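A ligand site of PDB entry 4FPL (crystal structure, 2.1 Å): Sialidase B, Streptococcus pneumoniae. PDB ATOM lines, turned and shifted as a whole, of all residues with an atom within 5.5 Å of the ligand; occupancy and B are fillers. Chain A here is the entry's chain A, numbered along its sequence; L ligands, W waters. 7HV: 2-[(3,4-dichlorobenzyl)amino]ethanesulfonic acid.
The side-chain hydroxyl of Tyr 653 sits at hydrogen-bond distance from the guanidinium group of Arg 557.
The side-chain amide oxygen (OD1) of Asn 457 sits at hydrogen-bond distance from the side-chain hydroxyl (OH) of Tyr 489 (3.4 Å).
The backbone NH (N) of Asp 344 lies within hydrogen-bond range of the backbone carbonyl oxygen (O) of Ile 326, at 2.9 Å.
The backbone carbonyl oxygen (O) of Gly 590 lies close to the guanidinium group (NH2) of Arg 557, at 3.3 Å.
OE2 of Glu 541 lies within salt-bridge range of NH1 of Arg 557 (2.9 Å).
O of Asp 327 sits at hydrogen-bond distance from N of Asp 344 (3.5 Å).
OD2 of Asp 270 is in salt-bridge range of NH1 of Arg 245 (3.9 Å).
The guanidinium group (NH2) of Arg 245 sits at hydrogen-bond distance from the side-chain hydroxyl (OG) of Ser 673.
An oxygen (OAC) of the ligand sits close to the side-chain hydroxyl of Tyr 653, at 3.3 Å.
The guanidinium group (NH1) of Arg 557 lies within salt-bridge range of an oxygen (OAC) of the ligand, 2.9 Å away.
The guanidinium group of Arg 245 is in salt-bridge range of an oxygen (OAA) of the ligand (3.0 Å).
The side-chain carboxylate (OD1) of Asp 270 is in salt-bridge range of a nitrogen (NAL) of the ligand, at 2.8 Å.
OAC of the ligand is in salt-bridge range of NH2 of Arg 619 (2.7 Å).
Water W2 lies within hydrogen-bond range of NAL of the ligand and OD1 of Asp 327.
Water W3 lies within hydrogen-bond range of the side-chain carboxylate of Glu 541, the side-chain hydroxyl of Tyr 509 and the side-chain carboxylate of Asp 327.
Water W1 lies within hydrogen-bond range of OD2 of Asp 344 (2.4 Å) and OD2 of Asp 327 (2.5 Å).
Ser 271 touches the ligand (O to CLE, 3.1 Å).
CG2 of Ile 326 touches CLD of the ligand, 3.5 Å away.
Asp 327 touches the ligand (OD2 to CAF, 3.2 Å).
OD2 of Asp 344 touches CAG of the ligand, at 3.4 Å.
Met 346 touches the ligand (SD to CLD, 3.1 Å).
Gly 351 touches the ligand.
N of Asn 352 touches CLE of the ligand, at 3.0 Å.
Tyr 489 touches the ligand.
Tyr 509 touches the ligand (OH to CAK, 3.8 Å).
Ser 673 touches the ligand (O to OAA, 3.9 Å).
CZ3 of Trp 674 touches OAB of the ligand (3.5 Å).
Within 4 Å of the ligand: Arg 245, Asp 270, Ser 271, Ile 326, Asp 327, Asp 344, Met 346, Gly 351, Asn 352, Tyr 489, Tyr 509, Arg 557, Arg 619, Tyr 653, Ser 673 and Trp 674.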
ATOM      1  N   ARG A 245       4.642  -3.975  -0.312  1.00  0.00           N
ATOM      2  CA  ARG A 245       3.775  -2.840  -0.571  1.00  0.00           C
ATOM      3  C   ARG A 245       4.040  -2.318  -1.970  1.00  0.00           C
ATOM      4  O   ARG A 245       5.029  -2.686  -2.601  1.00  0.00           O
ATOM      5  CB  ARG A 245       4.000  -1.734   0.464  1.00  0.00           C
ATOM      6  CG  ARG A 245       3.249  -1.902   1.795  1.00  0.00           C
ATOM      7  CD  ARG A 245       3.023  -0.515   2.466  1.00  0.00           C
ATOM      8  NE  ARG A 245       2.210   0.351   1.616  1.00  0.00           N
ATOM      9  CZ  ARG A 245       2.008   1.650   1.856  1.00  0.00           C
ATOM     10  NH1 ARG A 245       2.566   2.235   2.931  1.00  0.00           N
ATOM     11  NH2 ARG A 245       1.259   2.364   1.022  1.00  0.00           N
ATOM     12  N   ILE A 246       3.144  -1.445  -2.421  1.00  0.00           N
ATOM     13  CA  ILE A 246       3.331  -0.718  -3.673  1.00  0.00           C
ATOM     14  C   ILE A 246       3.325  -1.626  -4.904  1.00  0.00           C
ATOM     15  O   ILE A 246       4.336  -1.702  -5.615  1.00  0.00           O
ATOM     16  CB  ILE A 246       4.610   0.182  -3.651  1.00  0.00           C
ATOM     17  CG1 ILE A 246       4.875   0.785  -2.253  1.00  0.00           C
ATOM     18  CG2 ILE A 246       4.475   1.291  -4.646  1.00  0.00           C
ATOM     19  CD1 ILE A 246       3.769   1.723  -1.737  1.00  0.00           C
ATOM     20  N   ASP A 270       7.863   2.623   5.132  1.00  0.00           N
ATOM     21  CA  ASP A 270       8.572   3.285   4.028  1.00  0.00           C
ATOM     22  C   ASP A 270      10.029   3.420   4.449  1.00  0.00           C
ATOM     23  O   ASP A 270      10.338   3.418   5.643  1.00  0.00           O
ATOM     24  CB  ASP A 270       8.051   4.724   3.814  1.00  0.00           C
ATOM     25  CG  ASP A 270       6.710   4.794   3.075  1.00  0.00           C
ATOM     26  OD1 ASP A 270       6.237   5.938   2.886  1.00  0.00           O
ATOM     27  OD2 ASP A 270       6.147   3.744   2.661  1.00  0.00           O
ATOM     28  N   SER A 271      10.943   3.558   3.487  1.00  0.00           N
ATOM     29  CA  SER A 271      12.318   3.944   3.835  1.00  0.00           C
ATOM     30  C   SER A 271      12.329   5.093   4.885  1.00  0.00           C
ATOM     31  O   SER A 271      11.495   5.993   4.821  1.00  0.00           O
ATOM     32  CB  SER A 271      13.074   4.360   2.576  1.00  0.00           C
ATOM     33  OG  SER A 271      13.083   3.328   1.614  1.00  0.00           O
ATOM     34  N   LYS A 272      13.250   5.080   5.859  1.00  0.00           N
ATOM     35  CA  LYS A 272      14.383   4.139   5.944  1.00  0.00           C
ATOM     36  C   LYS A 272      14.034   2.718   6.417  1.00  0.00           C
ATOM     37  O   LYS A 272      13.305   2.495   7.407  1.00  0.00           O
ATOM     38  CB  LYS A 272      15.485   4.730   6.841  1.00  0.00           C
ATOM     39  CG  LYS A 272      15.061   4.916   8.291  1.00  0.00           C
ATOM     40  CD  LYS A 272      16.155   5.571   9.122  1.00  0.00           C
ATOM     41  CE  LYS A 272      15.679   5.742  10.577  1.00  0.00           C
ATOM     42  NZ  LYS A 272      16.761   6.201  11.513  1.00  0.00           N
ATOM     43  N   ILE A 326      12.364   2.151  -3.326  1.00  0.00           N
ATOM     44  CA  ILE A 326      10.964   2.312  -2.956  1.00  0.00           C
ATOM     45  C   ILE A 326      10.214   2.899  -4.128  1.00  0.00           C
ATOM     46  O   ILE A 326      10.759   3.722  -4.866  1.00  0.00           O
ATOM     47  CB  ILE A 326      10.810   3.195  -1.674  1.00  0.00           C
ATOM     48  CG1 ILE A 326       9.345   3.361  -1.278  1.00  0.00           C
ATOM     49  CG2 ILE A 326      11.482   4.549  -1.829  1.00  0.00           C
ATOM     50  CD1 ILE A 326       9.186   4.032   0.124  1.00  0.00           C
ATOM     51  N   ASP A 327       8.963   2.479  -4.302  1.00  0.00           N
ATOM     52  CA  ASP A 327       8.091   2.978  -5.366  1.00  0.00           C
ATOM     53  C   ASP A 327       8.625   2.664  -6.763  1.00  0.00           C
ATOM     54  O   ASP A 327       9.384   3.451  -7.326  1.00  0.00           O
ATOM     55  CB  ASP A 327       7.874   4.490  -5.250  1.00  0.00           C
ATOM     56  CG  ASP A 327       7.047   4.891  -4.028  1.00  0.00           C
ATOM     57  OD1 ASP A 327       6.471   3.999  -3.367  1.00  0.00           O
ATOM     58  OD2 ASP A 327       6.966   6.111  -3.734  1.00  0.00           O
ATOM     59  N   ASP A 344      12.585   4.786  -6.884  1.00  0.00           N
ATOM     60  CA  ASP A 344      13.410   5.705  -6.097  1.00  0.00           C
ATOM     61  C   ASP A 344      14.543   4.888  -5.465  1.00  0.00           C
ATOM     62  O   ASP A 344      14.385   3.694  -5.203  1.00  0.00           O
ATOM     63  CB  ASP A 344      12.607   6.380  -4.978  1.00  0.00           C
ATOM     64  CG  ASP A 344      11.370   7.127  -5.476  1.00  0.00           C
ATOM     65  OD1 ASP A 344      11.400   7.720  -6.587  1.00  0.00           O
ATOM     66  OD2 ASP A 344      10.356   7.151  -4.749  1.00  0.00           O
ATOM     67  N   MET A 346      17.508   5.148  -2.175  1.00  0.00           N
ATOM     68  CA  MET A 346      17.956   5.833  -0.962  1.00  0.00           C
ATOM     69  C   MET A 346      19.274   5.253  -0.498  1.00  0.00           C
ATOM     70  O   MET A 346      19.396   4.032  -0.346  1.00  0.00           O
ATOM     71  CB  MET A 346      16.987   5.545   0.191  1.00  0.00           C
ATOM     72  CG  MET A 346      15.528   5.542  -0.129  1.00  0.00           C
ATOM     73  SD  MET A 346      14.876   7.086   0.447  1.00  0.00           S
ATOM     74  CE  MET A 346      15.137   7.969  -1.050  1.00  0.00           C
ATOM     75  N   GLY A 351      15.370   8.189   4.161  1.00  0.00           N
ATOM     76  CA  GLY A 351      14.010   8.183   3.662  1.00  0.00           C
ATOM     77  C   GLY A 351      13.699   9.584   3.132  1.00  0.00           C
ATOM     78  O   GLY A 351      14.594  10.426   3.072  1.00  0.00           O
ATOM     79  N   ASN A 352      12.452   9.835   2.737  1.00  0.00           N
ATOM     80  CA  ASN A 352      12.100  11.187   2.331  1.00  0.00           C
ATOM     81  C   ASN A 352      12.164  12.148   3.527  1.00  0.00           C
ATOM     82  O   ASN A 352      12.386  13.351   3.370  1.00  0.00           O
ATOM     83  CB  ASN A 352      10.756  11.248   1.547  1.00  0.00           C
ATOM     84  CG  ASN A 352       9.494  11.271   2.435  1.00  0.00           C
ATOM     85  OD1 ASN A 352       9.544  11.513   3.643  1.00  0.00           O
ATOM     86  ND2 ASN A 352       8.340  11.042   1.807  1.00  0.00           N
ATOM     87  N   ASN A 353      11.969  11.584   4.723  1.00  0.00           N
ATOM     88  CA  ASN A 353      11.978  12.341   5.974  1.00  0.00           C
ATOM     89  C   ASN A 353      13.288  13.094   6.223  1.00  0.00           C
ATOM     90  O   ASN A 353      13.285  14.256   6.652  1.00  0.00           O
ATOM     91  CB  ASN A 353      11.694  11.408   7.159  1.00  0.00           C
ATOM     92  CG  ASN A 353      11.888  12.082   8.503  1.00  0.00           C
ATOM     93  OD1 ASN A 353      11.030  12.853   8.954  1.00  0.00           O
ATOM     94  ND2 ASN A 353      13.001  11.795   9.168  1.00  0.00           N
ATOM     95  N   ASN A 457      17.330  11.544  -2.029  1.00  0.00           N
ATOM     96  CA  ASN A 457      16.625  10.581  -2.881  1.00  0.00           C
ATOM     97  C   ASN A 457      17.012  10.704  -4.355  1.00  0.00           C
ATOM     98  O   ASN A 457      17.128  11.808  -4.885  1.00  0.00           O
ATOM     99  CB  ASN A 457      15.107  10.745  -2.724  1.00  0.00           C
ATOM    100  CG  ASN A 457      14.639  12.130  -3.094  1.00  0.00           C
ATOM    101  OD1 ASN A 457      14.910  13.100  -2.383  1.00  0.00           O
ATOM    102  ND2 ASN A 457      13.961  12.238  -4.243  1.00  0.00           N
ATOM    103  N   TYR A 489       9.985  12.541  -6.920  1.00  0.00           N
ATOM    104  CA  TYR A 489       9.590  11.221  -6.458  1.00  0.00           C
ATOM    105  C   TYR A 489       8.795  10.462  -7.539  1.00  0.00           C
ATOM    106  O   TYR A 489       7.808  10.973  -8.059  1.00  0.00           O
ATOM    107  CB  TYR A 489       8.764  11.351  -5.171  1.00  0.00           C
ATOM    108  CG  TYR A 489       9.595  11.793  -3.996  1.00  0.00           C
ATOM    109  CD1 TYR A 489      10.335  10.885  -3.264  1.00  0.00           C
ATOM    110  CD2 TYR A 489       9.650  13.133  -3.639  1.00  0.00           C
ATOM    111  CE1 TYR A 489      11.111  11.276  -2.196  1.00  0.00           C
ATOM    112  CE2 TYR A 489      10.425  13.545  -2.562  1.00  0.00           C
ATOM    113  CZ  TYR A 489      11.156  12.610  -1.849  1.00  0.00           C
ATOM    114  OH  TYR A 489      11.931  13.007  -0.774  1.00  0.00           O
ATOM    115  N   TYR A 509       6.652  13.356  -8.891  1.00  0.00           N
ATOM    116  CA  TYR A 509       6.134  14.545  -8.203  1.00  0.00           C
ATOM    117  C   TYR A 509       7.190  15.196  -7.321  1.00  0.00           C
ATOM    118  O   TYR A 509       8.141  14.556  -6.857  1.00  0.00           O
ATOM    119  CB  TYR A 509       4.874  14.236  -7.394  1.00  0.00           C
ATOM    120  CG  TYR A 509       5.091  13.273  -6.247  1.00  0.00           C
ATOM    121  CD1 TYR A 509       5.305  13.730  -4.945  1.00  0.00           C
ATOM    122  CD2 TYR A 509       5.063  11.902  -6.459  1.00  0.00           C
ATOM    123  CE1 TYR A 509       5.490  12.850  -3.896  1.00  0.00           C
ATOM    124  CE2 TYR A 509       5.247  11.008  -5.411  1.00  0.00           C
ATOM    125  CZ  TYR A 509       5.465  11.488  -4.128  1.00  0.00           C
ATOM    126  OH  TYR A 509       5.649  10.594  -3.080  1.00  0.00           O
ATOM    127  N   THR A 539       1.873  14.409  -1.588  1.00  0.00           N
ATOM    128  CA  THR A 539       2.296  13.141  -2.135  1.00  0.00           C
ATOM    129  C   THR A 539       1.419  12.933  -3.364  1.00  0.00           C
ATOM    130  O   THR A 539       0.450  12.180  -3.335  1.00  0.00           O
ATOM    131  CB  THR A 539       2.099  12.017  -1.094  1.00  0.00           C
ATOM    132  OG1 THR A 539       2.740  12.407   0.125  1.00  0.00           O
ATOM    133  CG2 THR A 539       2.683  10.683  -1.578  1.00  0.00           C
ATOM    134  N   GLU A 541       0.852  11.339  -6.056  1.00  0.00           N
ATOM    135  CA  GLU A 541       1.049  10.149  -6.890  1.00  0.00           C
ATOM    136  C   GLU A 541       0.067  10.177  -8.052  1.00  0.00           C
ATOM    137  O   GLU A 541      -1.159  10.267  -7.835  1.00  0.00           O
ATOM    138  CB  GLU A 541       0.899   8.876  -6.045  1.00  0.00           C
ATOM    139  CG  GLU A 541       2.005   8.703  -4.993  1.00  0.00           C
ATOM    140  CD  GLU A 541       1.539   7.905  -3.787  1.00  0.00           C
ATOM    141  OE1 GLU A 541       2.397   7.383  -3.029  1.00  0.00           O
ATOM    142  OE2 GLU A 541       0.310   7.785  -3.593  1.00  0.00           O
ATOM    143  N   ARG A 557      -3.375  11.827  -6.715  1.00  0.00           N
ATOM    144  CA  ARG A 557      -3.666  11.935  -5.288  1.00  0.00           C
ATOM    145  C   ARG A 557      -3.413  13.367  -4.824  1.00  0.00           C
ATOM    146  O   ARG A 557      -2.480  14.013  -5.288  1.00  0.00           O
ATOM    147  CB  ARG A 557      -2.729  10.972  -4.537  1.00  0.00           C
ATOM    148  CG  ARG A 557      -2.667  11.130  -3.026  1.00  0.00           C
ATOM    149  CD  ARG A 557      -1.738  10.071  -2.432  1.00  0.00           C
ATOM    150  NE  ARG A 557      -1.522  10.258  -1.001  1.00  0.00           N
ATOM    151  CZ  ARG A 557      -0.782   9.453  -0.250  1.00  0.00           C
ATOM    152  NH1 ARG A 557      -0.184   8.388  -0.783  1.00  0.00           N
ATOM    153  NH2 ARG A 557      -0.644   9.713   1.046  1.00  0.00           N
ATOM    154  N   GLY A 590      -4.924  11.118   1.423  1.00  0.00           N
ATOM    155  CA  GLY A 590      -5.003  10.578   0.076  1.00  0.00           C
ATOM    156  C   GLY A 590      -4.414   9.179  -0.069  1.00  0.00           C
ATOM    157  O   GLY A 590      -3.741   8.678   0.841  1.00  0.00           O
ATOM    158  N   ARG A 619      -8.425   3.999   4.456  1.00  0.00           N
ATOM    159  CA  ARG A 619      -8.129   3.302   3.210  1.00  0.00           C
ATOM    160  C   ARG A 619      -8.929   2.008   3.221  1.00  0.00           C
ATOM    161  O   ARG A 619      -8.438   0.938   3.636  1.00  0.00           O
ATOM    162  CB  ARG A 619      -6.624   3.051   3.056  1.00  0.00           C
ATOM    163  CG  ARG A 619      -5.794   4.352   2.978  1.00  0.00           C
ATOM    164  CD  ARG A 619      -4.308   4.117   2.693  1.00  0.00           C
ATOM    165  NE  ARG A 619      -3.631   5.335   2.221  1.00  0.00           N
ATOM    166  CZ  ARG A 619      -2.310   5.476   2.153  1.00  0.00           C
ATOM    167  NH1 ARG A 619      -1.497   4.484   2.534  1.00  0.00           N
ATOM    168  NH2 ARG A 619      -1.780   6.622   1.707  1.00  0.00           N
ATOM    169  N   TYR A 653      -3.093   1.048  -1.763  1.00  0.00           N
ATOM    170  CA  TYR A 653      -2.421   1.183  -3.052  1.00  0.00           C
ATOM    171  C   TYR A 653      -2.866   0.054  -3.982  1.00  0.00           C
ATOM    172  O   TYR A 653      -3.153  -1.054  -3.522  1.00  0.00           O
ATOM    173  CB  TYR A 653      -0.907   1.148  -2.900  1.00  0.00           C
ATOM    174  CG  TYR A 653      -0.278   2.479  -2.525  1.00  0.00           C
ATOM    175  CD1 TYR A 653      -0.778   3.220  -1.458  1.00  0.00           C
ATOM    176  CD2 TYR A 653       0.826   2.975  -3.208  1.00  0.00           C
ATOM    177  CE1 TYR A 653      -0.213   4.431  -1.083  1.00  0.00           C
ATOM    178  CE2 TYR A 653       1.412   4.193  -2.837  1.00  0.00           C
ATOM    179  CZ  TYR A 653       0.892   4.907  -1.777  1.00  0.00           C
ATOM    180  OH  TYR A 653       1.455   6.110  -1.396  1.00  0.00           O
ATOM    181  N   SER A 673      -3.114   0.663   4.760  1.00  0.00           N
ATOM    182  CA  SER A 673      -1.668   0.839   4.874  1.00  0.00           C
ATOM    183  C   SER A 673      -1.300   2.216   5.436  1.00  0.00           C
ATOM    184  O   SER A 673      -0.128   2.605   5.458  1.00  0.00           O
ATOM    185  CB  SER A 673      -0.996   0.612   3.516  1.00  0.00           C
ATOM    186  OG  SER A 673      -1.447   1.556   2.561  1.00  0.00           O
ATOM    187  N   TRP A 674      -2.302   2.961   5.891  1.00  0.00           N
ATOM    188  CA  TRP A 674      -2.024   4.214   6.620  1.00  0.00           C
ATOM    189  C   TRP A 674      -2.115   3.963   8.119  1.00  0.00           C
ATOM    190  O   TRP A 674      -1.281   4.421   8.893  1.00  0.00           O
ATOM    191  CB  TRP A 674      -3.012   5.317   6.215  1.00  0.00           C
ATOM    192  CG  TRP A 674      -2.687   6.672   6.790  1.00  0.00           C
ATOM    193  CD1 TRP A 674      -3.176   7.225   7.946  1.00  0.00           C
ATOM    194  CD2 TRP A 674      -1.780   7.641   6.227  1.00  0.00           C
ATOM    195  NE1 TRP A 674      -2.633   8.477   8.141  1.00  0.00           N
ATOM    196  CE2 TRP A 674      -1.782   8.754   7.097  1.00  0.00           C
ATOM    197  CE3 TRP A 674      -0.971   7.674   5.078  1.00  0.00           C
ATOM    198  CZ2 TRP A 674      -1.001   9.903   6.851  1.00  0.00           C
ATOM    199  CZ3 TRP A 674      -0.210   8.810   4.827  1.00  0.00           C
ATOM    200  CH2 TRP A 674      -0.225   9.900   5.714  1.00  0.00           C
HETATM  201  CAH 7HV L   1       8.152   7.953   1.000  1.00  0.00           C
HETATM  202  CAO 7HV L   1       9.530   7.819   0.968  1.00  0.00           C
HETATM  203 CLE  7HV L   1      10.436   7.684   2.467  1.00  0.00          CL
HETATM  204  CAN 7HV L   1      10.190   7.814  -0.274  1.00  0.00           C
HETATM  205 CLD  7HV L   1      11.927   7.665  -0.271  1.00  0.00          CL
HETATM  206  CAG 7HV L   1       9.485   7.910  -1.507  1.00  0.00           C
HETATM  207  CAF 7HV L   1       8.095   8.029  -1.464  1.00  0.00           C
HETATM  208  CAM 7HV L   1       7.444   8.068  -0.210  1.00  0.00           C
HETATM  209  CAK 7HV L   1       6.004   8.174  -0.112  1.00  0.00           C
HETATM  210  NAL 7HV L   1       5.400   6.971   0.474  1.00  0.00           N
HETATM  211  CAI 7HV L   1       4.052   7.236   0.857  1.00  0.00           C
HETATM  212  CAJ 7HV L   1       3.272   5.970   1.263  1.00  0.00           C
HETATM  213  SAP 7HV L   1       1.847   6.210   2.329  1.00  0.00           S
HETATM  214  OAC 7HV L   1       0.863   7.169   1.679  1.00  0.00           O
HETATM  215  OAB 7HV L   1       2.350   6.751   3.614  1.00  0.00           O
HETATM  216  OAA 7HV L   1       1.206   4.891   2.550  1.00  0.00           O
HETATM  217  O   HOH W   1       8.062   7.928  -4.959  1.00  0.00           O
HETATM  218  O   HOH W   2       4.857   4.988  -1.342  1.00  0.00           O
HETATM  219  O   HOH W   3       5.008   7.979  -3.360  1.00  0.00           O
